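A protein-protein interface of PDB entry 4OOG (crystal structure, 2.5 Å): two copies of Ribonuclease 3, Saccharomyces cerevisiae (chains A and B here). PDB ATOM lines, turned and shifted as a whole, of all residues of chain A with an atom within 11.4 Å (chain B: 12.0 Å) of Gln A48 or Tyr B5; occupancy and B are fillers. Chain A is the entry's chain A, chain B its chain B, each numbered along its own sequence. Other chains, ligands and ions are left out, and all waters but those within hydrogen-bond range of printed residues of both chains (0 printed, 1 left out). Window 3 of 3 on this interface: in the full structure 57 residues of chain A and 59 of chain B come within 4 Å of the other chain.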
ATOM      1  N   LEU A  28      24.943   6.171  20.146  1.00  0.00           N
ATOM      2  CA  LEU A  28      25.681   7.397  20.451  1.00  0.00           C
ATOM      3  C   LEU A  28      25.268   8.102  21.741  1.00  0.00           C
ATOM      4  O   LEU A  28      26.120   8.566  22.499  1.00  0.00           O
ATOM      5  CB  LEU A  28      25.594   8.381  19.283  1.00  0.00           C
ATOM      6  CG  LEU A  28      26.404   7.992  18.048  1.00  0.00           C
ATOM      7  CD1 LEU A  28      26.329   9.083  16.998  1.00  0.00           C
ATOM      8  CD2 LEU A  28      27.847   7.714  18.436  1.00  0.00           C
ATOM      9  N   SER A  29      23.966   8.192  21.985  1.00  0.00           N
ATOM     10  CA  SER A  29      23.474   8.960  23.122  1.00  0.00           C
ATOM     11  C   SER A  29      23.734   8.267  24.453  1.00  0.00           C
ATOM     12  O   SER A  29      23.615   7.049  24.560  1.00  0.00           O
ATOM     13  CB  SER A  29      21.980   9.260  22.978  1.00  0.00           C
ATOM     14  OG  SER A  29      21.514  10.050  24.059  1.00  0.00           O
ATOM     15  N   PRO A  30      24.122   9.052  25.466  1.00  0.00           N
ATOM     16  CA  PRO A  30      24.095   8.581  26.851  1.00  0.00           C
ATOM     17  C   PRO A  30      22.694   8.788  27.418  1.00  0.00           C
ATOM     18  O   PRO A  30      21.825   9.304  26.713  1.00  0.00           O
ATOM     19  CB  PRO A  30      25.094   9.506  27.547  1.00  0.00           C
ATOM     20  CG  PRO A  30      25.033  10.768  26.764  1.00  0.00           C
ATOM     21  CD  PRO A  30      24.778  10.366  25.337  1.00  0.00           C
ATOM     22  N   ALA A  38      25.237  17.583  32.466  1.00  0.00           N
ATOM     23  CA  ALA A  38      25.654  18.697  31.624  1.00  0.00           C
ATOM     24  C   ALA A  38      24.763  19.920  31.814  1.00  0.00           C
ATOM     25  O   ALA A  38      25.256  21.027  32.037  1.00  0.00           O
ATOM     26  CB  ALA A  38      25.675  18.275  30.165  1.00  0.00           C
ATOM     27  N   GLN A  42      26.652  23.997  33.685  1.00  0.00           N
ATOM     28  CA  GLN A  42      27.353  24.119  32.426  1.00  0.00           C
ATOM     29  C   GLN A  42      28.495  25.089  32.642  1.00  0.00           C
ATOM     30  O   GLN A  42      28.335  26.306  32.554  1.00  0.00           O
ATOM     31  CB  GLN A  42      26.390  24.643  31.361  1.00  0.00           C
ATOM     32  CG  GLN A  42      25.277  25.516  31.930  1.00  0.00           C
ATOM     33  CD  GLN A  42      23.955  25.324  31.211  1.00  0.00           C
ATOM     34  OE1 GLN A  42      23.818  25.670  30.038  1.00  0.00           O
ATOM     35  NE2 GLN A  42      22.975  24.766  31.912  1.00  0.00           N
ATOM     36  N   ASP A  43      29.658  24.512  32.915  1.00  0.00           N
ATOM     37  CA  ASP A  43      30.913  25.225  33.046  1.00  0.00           C
ATOM     38  C   ASP A  43      31.935  24.362  32.343  1.00  0.00           C
ATOM     39  O   ASP A  43      32.529  24.733  31.330  1.00  0.00           O
ATOM     40  CB  ASP A  43      31.285  25.369  34.520  1.00  0.00           C
ATOM     41  CG  ASP A  43      30.108  25.785  35.380  1.00  0.00           C
ATOM     42  OD1 ASP A  43      29.463  26.804  35.056  1.00  0.00           O
ATOM     43  OD2 ASP A  43      29.818  25.084  36.373  1.00  0.00           O
ATOM     44  N   ARG A  44      32.123  23.189  32.942  1.00  0.00           N
ATOM     45  CA  ARG A  44      33.005  22.143  32.455  1.00  0.00           C
ATOM     46  C   ARG A  44      32.639  21.732  31.036  1.00  0.00           C
ATOM     47  O   ARG A  44      33.505  21.326  30.260  1.00  0.00           O
ATOM     48  CB  ARG A  44      32.903  20.927  33.382  1.00  0.00           C
ATOM     49  CG  ARG A  44      33.977  19.871  33.181  1.00  0.00           C
ATOM     50  CD  ARG A  44      35.167  20.126  34.091  1.00  0.00           C
ATOM     51  NE  ARG A  44      36.222  19.130  33.920  1.00  0.00           N
ATOM     52  CZ  ARG A  44      37.354  19.119  34.615  1.00  0.00           C
ATOM     53  NH1 ARG A  44      37.580  20.051  35.532  1.00  0.00           N
ATOM     54  NH2 ARG A  44      38.263  18.178  34.394  1.00  0.00           N
ATOM     55  N   VAL A  45      31.356  21.831  30.698  1.00  0.00           N
ATOM     56  CA  VAL A  45      30.896  21.441  29.369  1.00  0.00           C
ATOM     57  C   VAL A  45      31.473  22.363  28.291  1.00  0.00           C
ATOM     58  O   VAL A  45      31.441  23.589  28.426  1.00  0.00           O
ATOM     59  CB  VAL A  45      29.346  21.353  29.276  1.00  0.00           C
ATOM     60  CG1 VAL A  45      28.801  20.441  30.366  1.00  0.00           C
ATOM     61  CG2 VAL A  45      28.707  22.724  29.373  1.00  0.00           C
ATOM     62  N   PRO A  46      32.037  21.766  27.228  1.00  0.00           N
ATOM     63  CA  PRO A  46      32.660  22.507  26.124  1.00  0.00           C
ATOM     64  C   PRO A  46      31.732  23.548  25.499  1.00  0.00           C
ATOM     65  O   PRO A  46      30.516  23.366  25.464  1.00  0.00           O
ATOM     66  CB  PRO A  46      33.018  21.408  25.110  1.00  0.00           C
ATOM     67  CG  PRO A  46      32.305  20.168  25.578  1.00  0.00           C
ATOM     68  CD  PRO A  46      32.175  20.311  27.057  1.00  0.00           C
ATOM     69  N   VAL A  47      32.324  24.635  25.016  1.00  0.00           N
ATOM     70  CA  VAL A  47      31.575  25.771  24.494  1.00  0.00           C
ATOM     71  C   VAL A  47      30.795  25.422  23.230  1.00  0.00           C
ATOM     72  O   VAL A  47      29.719  25.970  22.984  1.00  0.00           O
ATOM     73  CB  VAL A  47      32.518  26.956  24.194  1.00  0.00           C
ATOM     74  CG1 VAL A  47      31.723  28.200  23.825  1.00  0.00           C
ATOM     75  CG2 VAL A  47      33.417  27.228  25.390  1.00  0.00           C
ATOM     76  N   GLN A  48      31.334  24.503  22.435  1.00  0.00           N
ATOM     77  CA  GLN A  48      30.728  24.161  21.153  1.00  0.00           C
ATOM     78  C   GLN A  48      29.382  23.453  21.299  1.00  0.00           C
ATOM     79  O   GLN A  48      28.507  23.596  20.448  1.00  0.00           O
ATOM     80  CB  GLN A  48      31.680  23.309  20.307  1.00  0.00           C
ATOM     81  CG  GLN A  48      33.057  23.917  20.103  1.00  0.00           C
ATOM     82  CD  GLN A  48      34.035  23.509  21.187  1.00  0.00           C
ATOM     83  OE1 GLN A  48      33.745  22.633  22.001  1.00  0.00           O
ATOM     84  NE2 GLN A  48      35.204  24.140  21.199  1.00  0.00           N
ATOM     85  N   ILE A  49      29.217  22.694  22.378  1.00  0.00           N
ATOM     86  CA  ILE A  49      28.007  21.896  22.552  1.00  0.00           C
ATOM     87  C   ILE A  49      26.889  22.657  23.259  1.00  0.00           C
ATOM     88  O   ILE A  49      25.756  22.184  23.320  1.00  0.00           O
ATOM     89  CB  ILE A  49      28.286  20.599  23.332  1.00  0.00           C
ATOM     90  CG1 ILE A  49      28.435  20.899  24.823  1.00  0.00           C
ATOM     91  CG2 ILE A  49      29.520  19.894  22.780  1.00  0.00           C
ATOM     92  CD1 ILE A  49      28.500  19.662  25.688  1.00  0.00           C
ATOM     93  N   LEU A  50      27.214  23.829  23.796  1.00  0.00           N
ATOM     94  CA  LEU A  50      26.245  24.632  24.546  1.00  0.00           C
ATOM     95  C   LEU A  50      24.923  24.940  23.826  1.00  0.00           C
ATOM     96  O   LEU A  50      23.856  24.782  24.419  1.00  0.00           O
ATOM     97  CB  LEU A  50      26.884  25.921  25.074  1.00  0.00           C
ATOM     98  CG  LEU A  50      27.645  25.775  26.389  1.00  0.00           C
ATOM     99  CD1 LEU A  50      28.211  27.114  26.826  1.00  0.00           C
ATOM    100  CD2 LEU A  50      26.729  25.202  27.459  1.00  0.00           C
ATOM    101  N   PRO A  51      24.979  25.385  22.554  1.00  0.00           N
ATOM    102  CA  PRO A  51      23.705  25.639  21.870  1.00  0.00           C
ATOM    103  C   PRO A  51      22.827  24.395  21.714  1.00  0.00           C
ATOM    104  O   PRO A  51      21.610  24.529  21.601  1.00  0.00           O
ATOM    105  CB  PRO A  51      24.137  26.164  20.494  1.00  0.00           C
ATOM    106  CG  PRO A  51      25.564  25.750  20.343  1.00  0.00           C
ATOM    107  CD  PRO A  51      26.128  25.786  21.723  1.00  0.00           C
ATOM    108  N   SER A  52      23.436  23.212  21.717  1.00  0.00           N
ATOM    109  CA  SER A  52      22.689  21.964  21.585  1.00  0.00           C
ATOM    110  C   SER A  52      21.785  21.741  22.791  1.00  0.00           C
ATOM    111  O   SER A  52      20.693  21.186  22.671  1.00  0.00           O
ATOM    112  CB  SER A  52      23.644  20.779  21.431  1.00  0.00           C
ATOM    113  OG  SER A  52      24.602  21.020  20.416  1.00  0.00           O
ATOM    114  N   LEU A  53      22.251  22.185  23.955  1.00  0.00           N
ATOM    115  CA  LEU A  53      21.505  22.028  25.197  1.00  0.00           C
ATOM    116  C   LEU A  53      20.261  22.910  25.226  1.00  0.00           C
ATOM    117  O   LEU A  53      19.376  22.722  26.061  1.00  0.00           O
ATOM    118  CB  LEU A  53      22.402  22.337  26.397  1.00  0.00           C
ATOM    119  CG  LEU A  53      23.584  21.386  26.590  1.00  0.00           C
ATOM    120  CD1 LEU A  53      24.422  21.800  27.789  1.00  0.00           C
ATOM    121  CD2 LEU A  53      23.095  19.954  26.745  1.00  0.00           C
ATOM    122  N   SER A  54      20.203  23.877  24.316  1.00  0.00           N
ATOM    123  CA  SER A  54      19.038  24.747  24.193  1.00  0.00           C
ATOM    124  C   SER A  54      18.080  24.223  23.130  1.00  0.00           C
ATOM    125  O   SER A  54      17.068  24.855  22.827  1.00  0.00           O
ATOM    126  CB  SER A  54      19.464  26.180  23.869  1.00  0.00           C
ATOM    127  OG  SER A  54      20.375  26.210  22.785  1.00  0.00           O
ATOM    128  N   ARG A  55      18.415  23.070  22.559  1.00  0.00           N
ATOM    129  CA  ARG A  55      17.567  22.431  21.561  1.00  0.00           C
ATOM    130  C   ARG A  55      17.077  21.069  22.038  1.00  0.00           C
ATOM    131  O   ARG A  55      17.729  20.411  22.853  1.00  0.00           O
ATOM    132  CB  ARG A  55      18.299  22.304  20.225  1.00  0.00           C
ATOM    133  CG  ARG A  55      18.571  23.638  19.555  1.00  0.00           C
ATOM    134  CD  ARG A  55      19.144  23.451  18.165  1.00  0.00           C
ATOM    135  NE  ARG A  55      20.438  22.776  18.194  1.00  0.00           N
ATOM    136  CZ  ARG A  55      21.604  23.407  18.287  1.00  0.00           C
ATOM    137  NH1 ARG A  55      21.639  24.730  18.364  1.00  0.00           N
ATOM    138  NH2 ARG A  55      22.736  22.715  18.305  1.00  0.00           N
ATOM    139  N   LEU A  58      18.983  16.766  21.761  1.00  0.00           N
ATOM    140  CA  LEU A  58      19.880  16.090  22.695  1.00  0.00           C
ATOM    141  C   LEU A  58      19.159  15.477  23.890  1.00  0.00           C
ATOM    142  O   LEU A  58      19.538  14.408  24.369  1.00  0.00           O
ATOM    143  CB  LEU A  58      20.984  17.030  23.181  1.00  0.00           C
ATOM    144  CG  LEU A  58      22.345  16.831  22.518  1.00  0.00           C
ATOM    145  CD1 LEU A  58      23.436  17.488  23.348  1.00  0.00           C
ATOM    146  CD2 LEU A  58      22.634  15.351  22.308  1.00  0.00           C
ATOM    147  N   SER B   1      36.724  12.799  28.371  1.00  0.00           N
ATOM    148  CA  SER B   1      35.515  13.464  28.843  1.00  0.00           C
ATOM    149  C   SER B   1      34.263  12.812  28.263  1.00  0.00           C
ATOM    150  O   SER B   1      34.331  11.744  27.655  1.00  0.00           O
ATOM    151  CB  SER B   1      35.551  14.953  28.487  1.00  0.00           C
ATOM    152  OG  SER B   1      34.427  15.637  29.017  1.00  0.00           O
ATOM    153  N   ASN B   2      33.122  13.466  28.456  1.00  0.00           N
ATOM    154  CA  ASN B   2      31.844  12.968  27.959  1.00  0.00           C
ATOM    155  C   ASN B   2      31.251  13.940  26.943  1.00  0.00           C
ATOM    156  O   ASN B   2      31.595  15.123  26.942  1.00  0.00           O
ATOM    157  CB  ASN B   2      30.875  12.754  29.127  1.00  0.00           C
ATOM    158  CG  ASN B   2      29.549  12.156  28.690  1.00  0.00           C
ATOM    159  OD1 ASN B   2      29.450  11.542  27.627  1.00  0.00           O
ATOM    160  ND2 ASN B   2      28.522  12.334  29.513  1.00  0.00           N
ATOM    161  N   TYR B   3      30.372  13.435  26.078  1.00  0.00           N
ATOM    162  CA  TYR B   3      29.681  14.263  25.089  1.00  0.00           C
ATOM    163  C   TYR B   3      30.630  14.981  24.127  1.00  0.00           C
ATOM    164  O   TYR B   3      30.805  16.195  24.207  1.00  0.00           O
ATOM    165  CB  TYR B   3      28.767  15.285  25.778  1.00  0.00           C
ATOM    166  CG  TYR B   3      27.308  14.884  25.847  1.00  0.00           C
ATOM    167  CD1 TYR B   3      26.713  14.165  24.820  1.00  0.00           C
ATOM    168  CD2 TYR B   3      26.525  15.235  26.939  1.00  0.00           C
ATOM    169  CE1 TYR B   3      25.378  13.805  24.879  1.00  0.00           C
ATOM    170  CE2 TYR B   3      25.190  14.879  27.009  1.00  0.00           C
ATOM    171  CZ  TYR B   3      24.621  14.164  25.978  1.00  0.00           C
ATOM    172  OH  TYR B   3      23.294  13.807  26.046  1.00  0.00           O
ATOM    173  N   LYS B   4      31.251  14.221  23.229  1.00  0.00           N
ATOM    174  CA  LYS B   4      32.102  14.799  22.193  1.00  0.00           C
ATOM    175  C   LYS B   4      31.243  15.620  21.239  1.00  0.00           C
ATOM    176  O   LYS B   4      30.078  15.296  21.013  1.00  0.00           O
ATOM    177  CB  LYS B   4      32.825  13.703  21.410  1.00  0.00           C
ATOM    178  CG  LYS B   4      32.920  12.370  22.134  1.00  0.00           C
ATOM    179  CD  LYS B   4      33.886  12.423  23.305  1.00  0.00           C
ATOM    180  CE  LYS B   4      33.879  11.109  24.064  1.00  0.00           C
ATOM    181  NZ  LYS B   4      32.502  10.745  24.506  1.00  0.00           N
ATOM    182  N   TYR B   5      31.819  16.674  20.673  1.00  0.00           N
ATOM    183  CA  TYR B   5      31.068  17.581  19.808  1.00  0.00           C
ATOM    184  C   TYR B   5      30.636  16.932  18.495  1.00  0.00           C
ATOM    185  O   TYR B   5      29.502  17.114  18.053  1.00  0.00           O
ATOM    186  CB  TYR B   5      31.873  18.853  19.535  1.00  0.00           C
ATOM    187  CG  TYR B   5      31.327  19.705  18.410  1.00  0.00           C
ATOM    188  CD1 TYR B   5      30.218  20.521  18.601  1.00  0.00           C
ATOM    189  CD2 TYR B   5      31.929  19.702  17.159  1.00  0.00           C
ATOM    190  CE1 TYR B   5      29.721  21.303  17.574  1.00  0.00           C
ATOM    191  CE2 TYR B   5      31.440  20.480  16.127  1.00  0.00           C
ATOM    192  CZ  TYR B   5      30.337  21.278  16.339  1.00  0.00           C
ATOM    193  OH  TYR B   5      29.852  22.054  15.310  1.00  0.00           O
ATOM    194  N   LEU B   6      31.538  16.180  17.874  1.00  0.00           N
ATOM    195  CA  LEU B   6      31.235  15.513  16.611  1.00  0.00           C
ATOM    196  C   LEU B   6      30.096  14.512  16.768  1.00  0.00           C
ATOM    197  O   LEU B   6      29.299  14.315  15.851  1.00  0.00           O
ATOM    198  CB  LEU B   6      32.473  14.810  16.050  1.00  0.00           C
ATOM    199  CG  LEU B   6      33.509  15.667  15.316  1.00  0.00           C
ATOM    200  CD1 LEU B   6      32.843  16.502  14.228  1.00  0.00           C
ATOM    201  CD2 LEU B   6      34.300  16.550  16.279  1.00  0.00           C
ATOM    202  N   GLU B   7      30.025  13.885  17.937  1.00  0.00           N
ATOM    203  CA  GLU B   7      28.980  12.910  18.216  1.00  0.00           C
ATOM    204  C   GLU B   7      27.641  13.597  18.440  1.00  0.00           C
ATOM    205  O   GLU B   7      26.590  13.049  18.106  1.00  0.00           O
ATOM    206  CB  GLU B   7      29.354  12.065  19.431  1.00  0.00           C
ATOM    207  CG  GLU B   7      30.704  11.388  19.300  1.00  0.00           C
ATOM    208  CD  GLU B   7      30.712   9.990  19.880  1.00  0.00           C
ATOM    209  OE1 GLU B   7      30.512   9.848  21.105  1.00  0.00           O
ATOM    210  OE2 GLU B   7      30.908   9.029  19.107  1.00  0.00           O
ATOM    211  N   VAL B   8      27.687  14.798  19.009  1.00  0.00           N
ATOM    212  CA  VAL B   8      26.484  15.586  19.250  1.00  0.00           C
ATOM    213  C   VAL B   8      25.747  15.871  17.944  1.00  0.00           C
ATOM    214  O   VAL B   8      24.527  15.722  17.861  1.00  0.00           O
ATOM    215  CB  VAL B   8      26.818  16.919  19.958  1.00  0.00           C
ATOM    216  CG1 VAL B   8      25.650  17.890  19.867  1.00  0.00           C
ATOM    217  CG2 VAL B   8      27.199  16.669  21.409  1.00  0.00           C
ATOM    218  N   ILE B   9      26.501  16.266  16.924  1.00  0.00           N
ATOM    219  CA  ILE B   9      25.927  16.581  15.622  1.00  0.00           C
ATOM    220  C   ILE B   9      25.278  15.353  14.988  1.00  0.00           C
ATOM    221  O   ILE B   9      24.165  15.435  14.466  1.00  0.00           O
ATOM    222  CB  ILE B   9      26.989  17.156  14.665  1.00  0.00           C
ATOM    223  CG1 ILE B   9      27.758  18.295  15.338  1.00  0.00           C
ATOM    224  CG2 ILE B   9      26.342  17.626  13.375  1.00  0.00           C
ATOM    225  CD1 ILE B   9      26.876  19.412  15.856  1.00  0.00           C
ATOM    226  N   GLN B  10      25.971  14.219  15.040  1.00  0.00           N
ATOM    227  CA  GLN B  10      25.436  12.965  14.518  1.00  0.00           C
ATOM    228  C   GLN B  10      24.138  12.610  15.225  1.00  0.00           C
ATOM    229  O   GLN B  10      23.168  12.188  14.596  1.00  0.00           O
ATOM    230  CB  GLN B  10      26.432  11.828  14.723  1.00  0.00           C
ATOM    231  CG  GLN B  10      27.688  11.917  13.890  1.00  0.00           C
ATOM    232  CD  GLN B  10      28.611  10.743  14.139  1.00  0.00           C
ATOM    233  OE1 GLN B  10      29.468  10.790  15.022  1.00  0.00           O
ATOM    234  NE2 GLN B  10      28.433   9.674  13.371  1.00  0.00           N
ATOM    235  N   LEU B  11      24.142  12.780  16.542  1.00  0.00           N
ATOM    236  CA  LEU B  11      22.968  12.530  17.364  1.00  0.00           C
ATOM    237  C   LEU B  11      21.804  13.429  16.978  1.00  0.00           C
ATOM    238  O   LEU B  11      20.701  12.949  16.720  1.00  0.00           O
ATOM    239  CB  LEU B  11      23.307  12.739  18.836  1.00  0.00           C
ATOM    240  CG  LEU B  11      23.526  11.469  19.647  1.00  0.00           C
ATOM    241  CD1 LEU B  11      24.006  11.828  21.044  1.00  0.00           C
ATOM    242  CD2 LEU B  11      22.238  10.665  19.695  1.00  0.00           C
ATOM    243  N   GLU B  12      22.056  14.735  16.946  1.00  0.00           N
ATOM    244  CA  GLU B  12      21.020  15.714  16.639  1.00  0.00           C
ATOM    245  C   GLU B  12      20.408  15.449  15.270  1.00  0.00           C
ATOM    246  O   GLU B  12      19.197  15.567  15.084  1.00  0.00           O
ATOM    247  CB  GLU B  12      21.584  17.135  16.699  1.00  0.00           C
ATOM    248  CG  GLU B  12      21.860  17.643  18.107  1.00  0.00           C
ATOM    249  CD  GLU B  12      22.147  19.135  18.144  1.00  0.00           C
ATOM    250  OE1 GLU B  12      23.031  19.595  17.389  1.00  0.00           O
ATOM    251  OE2 GLU B  12      21.482  19.849  18.925  1.00  0.00           O
ATOM    252  N   HIS B  13      21.259  15.084  14.319  1.00  0.00           N
ATOM    253  CA  HIS B  13      20.809  14.756  12.976  1.00  0.00           C
ATOM    254  C   HIS B  13      19.977  13.477  13.001  1.00  0.00           C
ATOM    255  O   HIS B  13      18.913  13.410  12.383  1.00  0.00           O
ATOM    256  CB  HIS B  13      22.010  14.595  12.044  1.00  0.00           C
ATOM    257  CG  HIS B  13      21.655  14.588  10.591  1.00  0.00           C
ATOM    258  ND1 HIS B  13      20.449  14.118  10.118  1.00  0.00           N
ATOM    259  CD2 HIS B  13      22.350  15.001   9.503  1.00  0.00           C
ATOM    260  CE1 HIS B  13      20.417  14.237   8.802  1.00  0.00           C
ATOM    261  NE2 HIS B  13      21.559  14.771   8.405  1.00  0.00           N
ATOM    262  N   ALA B  14      20.465  12.470  13.722  1.00  0.00           N
ATOM    263  CA  ALA B  14      19.771  11.190  13.832  1.00  0.00           C
ATOM    264  C   ALA B  14      18.378  11.341  14.437  1.00  0.00           C
ATOM    265  O   ALA B  14      17.411  10.782  13.922  1.00  0.00           O
ATOM    266  CB  ALA B  14      20.594  10.207  14.646  1.00  0.00           C
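Gln A48 touches just one residue of chain B: Tyr B5. Of chain A, only Gln A48 (3.6 Å) comes within 4 Å of Tyr B5. Val A47 touches none of the printed residues of chain B. Leu A50 touches none of the printed residues of chain B. Lys B4 touches none of the printed residues of chain A. No residue of chain A comes within 4 Å of Leu B6. Of chain A, only Ser A52 (3.3 Å) comes within 4 Å of Val B8. Ile B9 touches none of the printed residues of chain A. Of the printed residues of chain A, Glu B7 touches Leu A28. Printed residues of chain A within 4 Å of Tyr B3: Pro A30 (3.5 Å). Printed residues of chain A within 4 Å of Gln B10: Leu A28. Printed residues of chain B within 4 Å of Leu A58: Leu B11. Of the printed residues of chain A, Glu B12 touches Ser A52 and Arg A55. The nearest printed residue of chain B that does not touch Gln A48 is Val B8 (6.4 Å). The nearest printed residue of chain A that does not touch Leu B11 is Pro A30 (4.6 Å).
Of the 19 printed residues of chain A, 7 touch a printed residue of chain B. Printed residues of chain A that touch a printed residue of chain B: Leu A28, Ser A29, Pro A30, Gln A48, Ser A52, Arg A55 and Leu A58. Hydrophobic or aromatic side chains of chain A within 4 Å of the printed part of chain B: Leu A28, Pro A30 and Leu A58. Of the 14 printed residues of chain B, 7 touch a printed residue of chain A. Hydrophobic or aromatic side chains of chain B within 4 Å of the printed part of chain A: Tyr B3, Tyr B5, Val B8 and Leu B11. Among the printed residues, Asp or Glu carboxylates within 4 Å of a Lys or Arg side-chain nitrogen of the other chain: Arg A55 with Glu B12.
Leu A28 touches Glu B7. Leu A28 touches Gln B10 (CD1 to CB, 3.6 Å). Leu B11 touches Leu A28. Ser A29 touches Leu B11 (CB to CD2, 3.6 Å). Tyr B3 touches Pro A30 (CZ to CG, 3.5 Å). Gln A48 touches Tyr B5 (CB to CD1, 3.6 Å). CG1 of Val B8 touches OG of Ser A52, at 3.3 Å. CB of Ser A52 touches OE2 of Glu B12, at 3.4 Å. CD2 of Leu A58 touches CD1 of Leu B11, at 3.99 Å.
O of Ile A49 sits close to OG of Ser A52 (3.3 Å). The guanidinium group (NH1) of Arg A55 sits at hydrogen-bond distance from the backbone carbonyl oxygen (O) of Pro A51 (3.2 Å). The guanidinium group (NH2) of Arg A55 lies within hydrogen-bond range of the side-chain hydroxyl (OG) of Ser A52.
The side-chain carboxylate (OE2) of Glu B12 is in salt-bridge range of the guanidinium group (NH2) of Arg A55.
No position is printed for both chains. Of the 10 pairs that touch across the chains among the printed residues, none has its exchanged pair printed and touching as well.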
